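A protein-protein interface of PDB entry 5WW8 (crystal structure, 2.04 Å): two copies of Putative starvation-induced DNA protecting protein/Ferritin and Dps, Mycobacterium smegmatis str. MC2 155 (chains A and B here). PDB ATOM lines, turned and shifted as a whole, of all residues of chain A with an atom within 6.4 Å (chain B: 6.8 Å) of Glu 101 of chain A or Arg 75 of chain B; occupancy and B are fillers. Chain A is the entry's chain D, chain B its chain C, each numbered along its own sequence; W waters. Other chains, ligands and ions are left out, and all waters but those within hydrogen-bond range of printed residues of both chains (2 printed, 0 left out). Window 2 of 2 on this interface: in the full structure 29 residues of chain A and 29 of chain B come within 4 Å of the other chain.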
ATOM      1  N   TRP A  42      17.449   0.687 -20.740  1.00  0.00           N
ATOM      2  CA  TRP A  42      16.258  -0.008 -21.227  1.00  0.00           C
ATOM      3  C   TRP A  42      15.982  -1.308 -20.486  1.00  0.00           C
ATOM      4  O   TRP A  42      14.823  -1.616 -20.173  1.00  0.00           O
ATOM      5  CB  TRP A  42      16.356  -0.306 -22.723  1.00  0.00           C
ATOM      6  CG  TRP A  42      16.509   0.896 -23.611  1.00  0.00           C
ATOM      7  CD1 TRP A  42      15.846   2.088 -23.513  1.00  0.00           C
ATOM      8  CD2 TRP A  42      17.353   0.998 -24.764  1.00  0.00           C
ATOM      9  NE1 TRP A  42      16.246   2.939 -24.515  1.00  0.00           N
ATOM     10  CE2 TRP A  42      17.171   2.300 -25.300  1.00  0.00           C
ATOM     11  CE3 TRP A  42      18.258   0.116 -25.393  1.00  0.00           C
ATOM     12  CZ2 TRP A  42      17.854   2.749 -26.452  1.00  0.00           C
ATOM     13  CZ3 TRP A  42      18.943   0.559 -26.534  1.00  0.00           C
ATOM     14  CH2 TRP A  42      18.735   1.873 -27.051  1.00  0.00           C
ATOM     15  N   ASN A  43      17.044  -2.062 -20.199  1.00  0.00           N
ATOM     16  CA  ASN A  43      16.890  -3.449 -19.757  1.00  0.00           C
ATOM     17  C   ASN A  43      17.008  -3.735 -18.264  1.00  0.00           C
ATOM     18  O   ASN A  43      16.817  -4.878 -17.836  1.00  0.00           O
ATOM     19  CB  ASN A  43      17.813  -4.359 -20.575  1.00  0.00           C
ATOM     20  CG  ASN A  43      17.328  -4.540 -21.999  1.00  0.00           C
ATOM     21  OD1 ASN A  43      16.122  -4.450 -22.272  1.00  0.00           O
ATOM     22  ND2 ASN A  43      18.258  -4.819 -22.916  1.00  0.00           N
ATOM     23  N   VAL A  44      17.313  -2.705 -17.476  1.00  0.00           N
ATOM     24  CA  VAL A  44      17.421  -2.848 -16.023  1.00  0.00           C
ATOM     25  C   VAL A  44      16.036  -3.119 -15.418  1.00  0.00           C
ATOM     26  O   VAL A  44      15.053  -2.490 -15.815  1.00  0.00           O
ATOM     27  CB  VAL A  44      18.136  -1.627 -15.362  1.00  0.00           C
ATOM     28  CG1 VAL A  44      17.311  -0.347 -15.460  1.00  0.00           C
ATOM     29  CG2 VAL A  44      18.508  -1.918 -13.915  1.00  0.00           C
ATOM     30  N   VAL A  45      15.970  -4.095 -14.506  1.00  0.00           N
ATOM     31  CA  VAL A  45      14.742  -4.431 -13.768  1.00  0.00           C
ATOM     32  C   VAL A  45      15.082  -4.711 -12.305  1.00  0.00           C
ATOM     33  O   VAL A  45      16.243  -4.997 -11.982  1.00  0.00           O
ATOM     34  CB  VAL A  45      13.982  -5.652 -14.353  1.00  0.00           C
ATOM     35  CG1 VAL A  45      13.395  -5.338 -15.728  1.00  0.00           C
ATOM     36  CG2 VAL A  45      14.869  -6.898 -14.405  1.00  0.00           C
ATOM     37  N   ALA A  99      23.495  -9.470 -22.787  1.00  0.00           N
ATOM     38  CA  ALA A  99      22.168  -9.340 -23.366  1.00  0.00           C
ATOM     39  C   ALA A  99      21.091  -9.513 -22.288  1.00  0.00           C
ATOM     40  O   ALA A  99      21.397  -9.845 -21.142  1.00  0.00           O
ATOM     41  CB  ALA A  99      21.989 -10.374 -24.480  1.00  0.00           C
ATOM     42  N   PHE A 100      19.836  -9.279 -22.675  1.00  0.00           N
ATOM     43  CA  PHE A 100      18.640  -9.556 -21.849  1.00  0.00           C
ATOM     44  C   PHE A 100      18.456  -8.602 -20.646  1.00  0.00           C
ATOM     45  O   PHE A 100      19.279  -7.710 -20.408  1.00  0.00           O
ATOM     46  CB  PHE A 100      18.565 -11.047 -21.418  1.00  0.00           C
ATOM     47  CG  PHE A 100      18.953 -12.027 -22.503  1.00  0.00           C
ATOM     48  CD1 PHE A 100      18.233 -12.101 -23.705  1.00  0.00           C
ATOM     49  CD2 PHE A 100      20.047 -12.887 -22.320  1.00  0.00           C
ATOM     50  CE1 PHE A 100      18.606 -13.003 -24.706  1.00  0.00           C
ATOM     51  CE2 PHE A 100      20.417 -13.793 -23.317  1.00  0.00           C
ATOM     52  CZ  PHE A 100      19.696 -13.850 -24.509  1.00  0.00           C
ATOM     53  N   GLU A 101      17.349  -8.788 -19.924  1.00  0.00           N
ATOM     54  CA  GLU A 101      17.058  -8.077 -18.683  1.00  0.00           C
ATOM     55  C   GLU A 101      18.115  -8.389 -17.644  1.00  0.00           C
ATOM     56  O   GLU A 101      18.563  -9.531 -17.540  1.00  0.00           O
ATOM     57  CB  GLU A 101      15.688  -8.487 -18.156  1.00  0.00           C
ATOM     58  CG  GLU A 101      14.533  -7.958 -18.990  1.00  0.00           C
ATOM     59  CD  GLU A 101      13.205  -8.594 -18.627  1.00  0.00           C
ATOM     60  OE1 GLU A 101      13.124  -9.847 -18.572  1.00  0.00           O
ATOM     61  OE2 GLU A 101      12.234  -7.834 -18.413  1.00  0.00           O
ATOM     62  N   ARG A 102      18.544  -7.370 -16.904  1.00  0.00           N
ATOM     63  CA  ARG A 102      19.519  -7.573 -15.834  1.00  0.00           C
ATOM     64  C   ARG A 102      19.004  -6.895 -14.584  1.00  0.00           C
ATOM     65  O   ARG A 102      18.332  -5.863 -14.668  1.00  0.00           O
ATOM     66  CB  ARG A 102      20.929  -7.036 -16.173  1.00  0.00           C
ATOM     67  CG  ARG A 102      21.437  -7.120 -17.616  1.00  0.00           C
ATOM     68  CD  ARG A 102      21.608  -8.533 -18.181  1.00  0.00           C
ATOM     69  NE  ARG A 102      22.479  -9.406 -17.403  1.00  0.00           N
ATOM     70  CZ  ARG A 102      22.873 -10.626 -17.779  1.00  0.00           C
ATOM     71  NH1 ARG A 102      22.494 -11.153 -18.933  1.00  0.00           N
ATOM     72  NH2 ARG A 102      23.673 -11.322 -16.992  1.00  0.00           N
ATOM     73  N   SER A 103      19.322  -7.470 -13.429  1.00  0.00           N
ATOM     74  CA  SER A 103      18.861  -6.927 -12.154  1.00  0.00           C
ATOM     75  C   SER A 103      19.573  -5.602 -11.874  1.00  0.00           C
ATOM     76  O   SER A 103      20.674  -5.355 -12.395  1.00  0.00           O
ATOM     77  CB  SER A 103      19.110  -7.927 -11.017  1.00  0.00           C
ATOM     78  OG  SER A 103      20.481  -7.920 -10.644  1.00  0.00           O
ATOM     79  N   ASP A 106      23.054  -6.146 -10.497  1.00  0.00           N
ATOM     80  CA  ASP A 106      23.941  -6.542 -11.599  1.00  0.00           C
ATOM     81  C   ASP A 106      24.330  -5.337 -12.441  1.00  0.00           C
ATOM     82  O   ASP A 106      25.494  -5.154 -12.776  1.00  0.00           O
ATOM     83  CB  ASP A 106      23.261  -7.598 -12.488  1.00  0.00           C
ATOM     84  CG  ASP A 106      24.247  -8.375 -13.372  1.00  0.00           C
ATOM     85  OD1 ASP A 106      25.463  -8.401 -13.078  1.00  0.00           O
ATOM     86  OD2 ASP A 106      23.792  -8.994 -14.361  1.00  0.00           O
ATOM     87  N   ILE B  70      11.352   3.411 -29.587  1.00  0.00           N
ATOM     88  CA  ILE B  70      11.168   2.014 -30.014  1.00  0.00           C
ATOM     89  C   ILE B  70      11.599   1.015 -28.932  1.00  0.00           C
ATOM     90  O   ILE B  70      10.854   0.090 -28.613  1.00  0.00           O
ATOM     91  CB  ILE B  70      11.840   1.732 -31.388  1.00  0.00           C
ATOM     92  CG1 ILE B  70      11.227   2.633 -32.485  1.00  0.00           C
ATOM     93  CG2 ILE B  70      11.800   0.235 -31.759  1.00  0.00           C
ATOM     94  CD1 ILE B  70       9.741   2.443 -32.770  1.00  0.00           C
ATOM     95  N   ALA B  71      12.778   1.237 -28.352  1.00  0.00           N
ATOM     96  CA  ALA B  71      13.317   0.350 -27.328  1.00  0.00           C
ATOM     97  C   ALA B  71      12.388   0.282 -26.116  1.00  0.00           C
ATOM     98  O   ALA B  71      12.125  -0.804 -25.589  1.00  0.00           O
ATOM     99  CB  ALA B  71      14.704   0.799 -26.919  1.00  0.00           C
ATOM    100  N   GLU B  72      11.863   1.438 -25.715  1.00  0.00           N
ATOM    101  CA  GLU B  72      10.938   1.519 -24.592  1.00  0.00           C
ATOM    102  C   GLU B  72       9.559   0.946 -24.897  1.00  0.00           C
ATOM    103  O   GLU B  72       8.927   0.399 -23.995  1.00  0.00           O
ATOM    104  CB  GLU B  72      10.860   2.953 -24.045  1.00  0.00           C
ATOM    105  CG  GLU B  72      12.218   3.390 -23.506  1.00  0.00           C
ATOM    106  CD  GLU B  72      12.191   4.494 -22.472  1.00  0.00           C
ATOM    107  OE1 GLU B  72      11.256   5.325 -22.458  1.00  0.00           O
ATOM    108  OE2 GLU B  72      13.159   4.526 -21.673  1.00  0.00           O
ATOM    109  N   ARG B  73       9.093   1.075 -26.144  1.00  0.00           N
ATOM    110  CA  ARG B  73       7.866   0.375 -26.597  1.00  0.00           C
ATOM    111  C   ARG B  73       8.043  -1.156 -26.507  1.00  0.00           C
ATOM    112  O   ARG B  73       7.148  -1.867 -26.034  1.00  0.00           O
ATOM    113  CB  ARG B  73       7.451   0.790 -28.022  1.00  0.00           C
ATOM    114  CG  ARG B  73       6.103   0.233 -28.485  1.00  0.00           C
ATOM    115  CD  ARG B  73       4.958   0.741 -27.609  1.00  0.00           C
ATOM    116  NE  ARG B  73       3.651   0.161 -27.945  1.00  0.00           N
ATOM    117  CZ  ARG B  73       2.682  -0.051 -27.048  1.00  0.00           C
ATOM    118  NH1 ARG B  73       2.872   0.248 -25.762  1.00  0.00           N
ATOM    119  NH2 ARG B  73       1.525  -0.583 -27.428  1.00  0.00           N
ATOM    120  N   MET B  74       9.205  -1.643 -26.940  1.00  0.00           N
ATOM    121  CA  MET B  74       9.572  -3.058 -26.767  1.00  0.00           C
ATOM    122  C   MET B  74       9.467  -3.461 -25.300  1.00  0.00           C
ATOM    123  O   MET B  74       8.802  -4.449 -24.982  1.00  0.00           O
ATOM    124  CB  MET B  74      10.978  -3.336 -27.314  1.00  0.00           C
ATOM    125  CG  MET B  74      11.084  -3.185 -28.823  1.00  0.00           C
ATOM    126  SD  MET B  74      12.759  -3.361 -29.461  1.00  0.00           S
ATOM    127  CE  MET B  74      12.933  -5.154 -29.381  1.00  0.00           C
ATOM    128  N   ARG B  75      10.081  -2.677 -24.413  1.00  0.00           N
ATOM    129  CA  ARG B  75      10.018  -2.931 -22.971  1.00  0.00           C
ATOM    130  C   ARG B  75       8.580  -2.966 -22.436  1.00  0.00           C
ATOM    131  O   ARG B  75       8.208  -3.868 -21.684  1.00  0.00           O
ATOM    132  CB  ARG B  75      10.834  -1.893 -22.192  1.00  0.00           C
ATOM    133  CG  ARG B  75      12.336  -1.898 -22.450  1.00  0.00           C
ATOM    134  CD  ARG B  75      12.985  -3.268 -22.264  1.00  0.00           C
ATOM    135  NE  ARG B  75      12.973  -3.702 -20.870  1.00  0.00           N
ATOM    136  CZ  ARG B  75      12.471  -4.850 -20.433  1.00  0.00           C
ATOM    137  NH1 ARG B  75      12.516  -5.120 -19.138  1.00  0.00           N
ATOM    138  NH2 ARG B  75      11.939  -5.724 -21.277  1.00  0.00           N
ATOM    139  N   ALA B  76       7.777  -1.987 -22.844  1.00  0.00           N
ATOM    140  CA  ALA B  76       6.380  -1.893 -22.426  1.00  0.00           C
ATOM    141  C   ALA B  76       5.583  -3.155 -22.814  1.00  0.00           C
ATOM    142  O   ALA B  76       4.777  -3.659 -22.032  1.00  0.00           O
ATOM    143  CB  ALA B  76       5.750  -0.632 -23.012  1.00  0.00           C
ATOM    144  N   LEU B  77       5.860  -3.679 -24.009  1.00  0.00           N
ATOM    145  CA  LEU B  77       5.208  -4.889 -24.512  1.00  0.00           C
ATOM    146  C   LEU B  77       5.964  -6.180 -24.186  1.00  0.00           C
ATOM    147  O   LEU B  77       5.679  -7.231 -24.772  1.00  0.00           O
ATOM    148  CB  LEU B  77       4.987  -4.773 -26.027  1.00  0.00           C
ATOM    149  CG  LEU B  77       4.141  -3.597 -26.531  1.00  0.00           C
ATOM    150  CD1 LEU B  77       4.188  -3.542 -28.047  1.00  0.00           C
ATOM    151  CD2 LEU B  77       2.700  -3.673 -26.053  1.00  0.00           C
ATOM    152  N   ASP B  78       6.934  -6.097 -23.272  1.00  0.00           N
ATOM    153  CA  ASP B  78       7.649  -7.276 -22.775  1.00  0.00           C
ATOM    154  C   ASP B  78       8.666  -7.878 -23.772  1.00  0.00           C
ATOM    155  O   ASP B  78       9.049  -9.034 -23.656  1.00  0.00           O
ATOM    156  CB  ASP B  78       6.639  -8.336 -22.290  1.00  0.00           C
ATOM    157  CG  ASP B  78       7.145  -9.135 -21.133  1.00  0.00           C
ATOM    158  OD1 ASP B  78       7.827  -8.559 -20.255  1.00  0.00           O
ATOM    159  OD2 ASP B  78       6.841 -10.345 -21.093  1.00  0.00           O
ATOM    160  N   ALA B  79       9.097  -7.083 -24.751  1.00  0.00           N
ATOM    161  CA  ALA B  79      10.216  -7.445 -25.621  1.00  0.00           C
ATOM    162  C   ALA B  79      11.521  -6.876 -25.041  1.00  0.00           C
ATOM    163  O   ALA B  79      11.494  -6.010 -24.163  1.00  0.00           O
ATOM    164  CB  ALA B  79       9.977  -6.945 -27.045  1.00  0.00           C
ATOM    165  N   VAL B  80      12.656  -7.379 -25.529  1.00  0.00           N
ATOM    166  CA  VAL B  80      13.964  -7.007 -24.997  1.00  0.00           C
ATOM    167  C   VAL B  80      14.848  -6.446 -26.126  1.00  0.00           C
ATOM    168  O   VAL B  80      15.287  -7.203 -27.004  1.00  0.00           O
ATOM    169  CB  VAL B  80      14.650  -8.194 -24.257  1.00  0.00           C
ATOM    170  CG1 VAL B  80      15.990  -7.762 -23.684  1.00  0.00           C
ATOM    171  CG2 VAL B  80      13.762  -8.736 -23.139  1.00  0.00           C
ATOM    172  N   PRO B  81      15.097  -5.115 -26.118  1.00  0.00           N
ATOM    173  CA  PRO B  81      15.936  -4.509 -27.151  1.00  0.00           C
ATOM    174  C   PRO B  81      17.394  -4.922 -27.032  1.00  0.00           C
ATOM    175  O   PRO B  81      17.874  -5.255 -25.938  1.00  0.00           O
ATOM    176  CB  PRO B  81      15.811  -3.003 -26.875  1.00  0.00           C
ATOM    177  CG  PRO B  81      15.469  -2.916 -25.429  1.00  0.00           C
ATOM    178  CD  PRO B  81      14.565  -4.093 -25.198  1.00  0.00           C
HETATM  179  O   HOH W   1      19.436  -7.912 -25.226  1.00  0.00           O
HETATM  180  O   HOH W   2      13.351  -2.640 -18.000  1.00  0.00           O
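NE of Arg 75 of chain B lies within hydrogen-bond range of O of Trp 42 of chain A (2.9 Å). NH1 of Arg 75 of chain B lies within salt-bridge range of OE2 of Glu 101 of chain A (2.8 Å). The backbone carbonyl oxygen (O) of Pro 81 of chain B sits at hydrogen-bond distance from the side-chain amide nitrogen (ND2) of Asn 43 of chain A (3.1 Å).
Printed residues of chain B within 4 Å of Asn 43 of chain A: Arg 75, Val 80 and Pro 81. Of the printed residues of chain B, Val 45 of chain A touches Arg 75. Glu 101 of chain A touches just one residue of chain B: Arg 75. Printed residues of chain A within 4 Å of Glu 72 of chain B: Trp 42. Of the printed residues of chain A, Arg 75 of chain B touches Trp 42 (2.9 Å), Asn 43 (3.4 Å), Val 45 (3.5 Å) and Glu 101 (2.8 Å). Printed residues of chain A within 4 Å of Val 80 of chain B: Asn 43 and Phe 100. Of the printed residues of chain A, Pro 81 of chain B touches Trp 42 (3.9 Å) and Asn 43 (3.1 Å). The nearest residue of chain A that does not touch Arg 75 of chain B is Val 44 of chain A (4.9 Å). The nearest printed residue of chain A that does not touch Glu 72 of chain B is Asn 43 of chain A (7.8 Å).
Of the 10 printed residues of chain A, 5 touch a printed residue of chain B. Printed residues of chain A that touch a printed residue of chain B: Trp 42, Asn 43, Val 45, Phe 100 and Glu 101. Hydrophobic or aromatic side chains of chain A that line the printed part of chain B: Trp 42 and Val 45. Along chain B the printed residues that touch a printed residue of chain A span positions 71 to 81. Among the printed residues, Asp or Glu carboxylates within 4 Å of a Lys or Arg side-chain nitrogen of the other chain: Glu 101 of chain A with Arg 75 of chain B (2.8 Å).
No position is printed for both chains. Of the 10 pairs that touch across the chains among the printed residues, none has its exchanged pair printed and touching as well.
Water W2 lies within hydrogen-bond range of the backbone carbonyl oxygen of Val 44 of chain A (2.8 Å), the backbone carbonyl oxygen of Trp 42 of chain A (2.8 Å) and the guanidinium group of Arg 75 of chain B (2.9 Å). Water W1 bridges the backbone NH of Phe 100 of chain A and the backbone carbonyl oxygen of Pro 81 of chain B.
O of Ala 79 of chain B is in hydrogen-bond range of NH2 of Arg 75 of chain B, 2.9 Å away. N of Arg 102 of chain A lies within hydrogen-bond range of O of Asn 43 of chain A, at 3.2 Å. The backbone NH (N) of Val 45 of chain A lies within hydrogen-bond range of the backbone carbonyl oxygen (O) of Arg 102 of chain A (3.0 Å).
Among the printed residues, pairs that only touch across the chains: Trp 42 of chain A with Ala 71 of chain B, Trp 42 of chain A with Glu 72 of chain B, Trp 42 of chain A with Pro 81 of chain B, Asn 43 of chain A with Arg 75 of chain B, Asn 43 of chain A with Val 80 of chain B, Val 45 of chain A with Arg 75 of chain B and Phe 100 of chain A with Val 80 of chain B.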
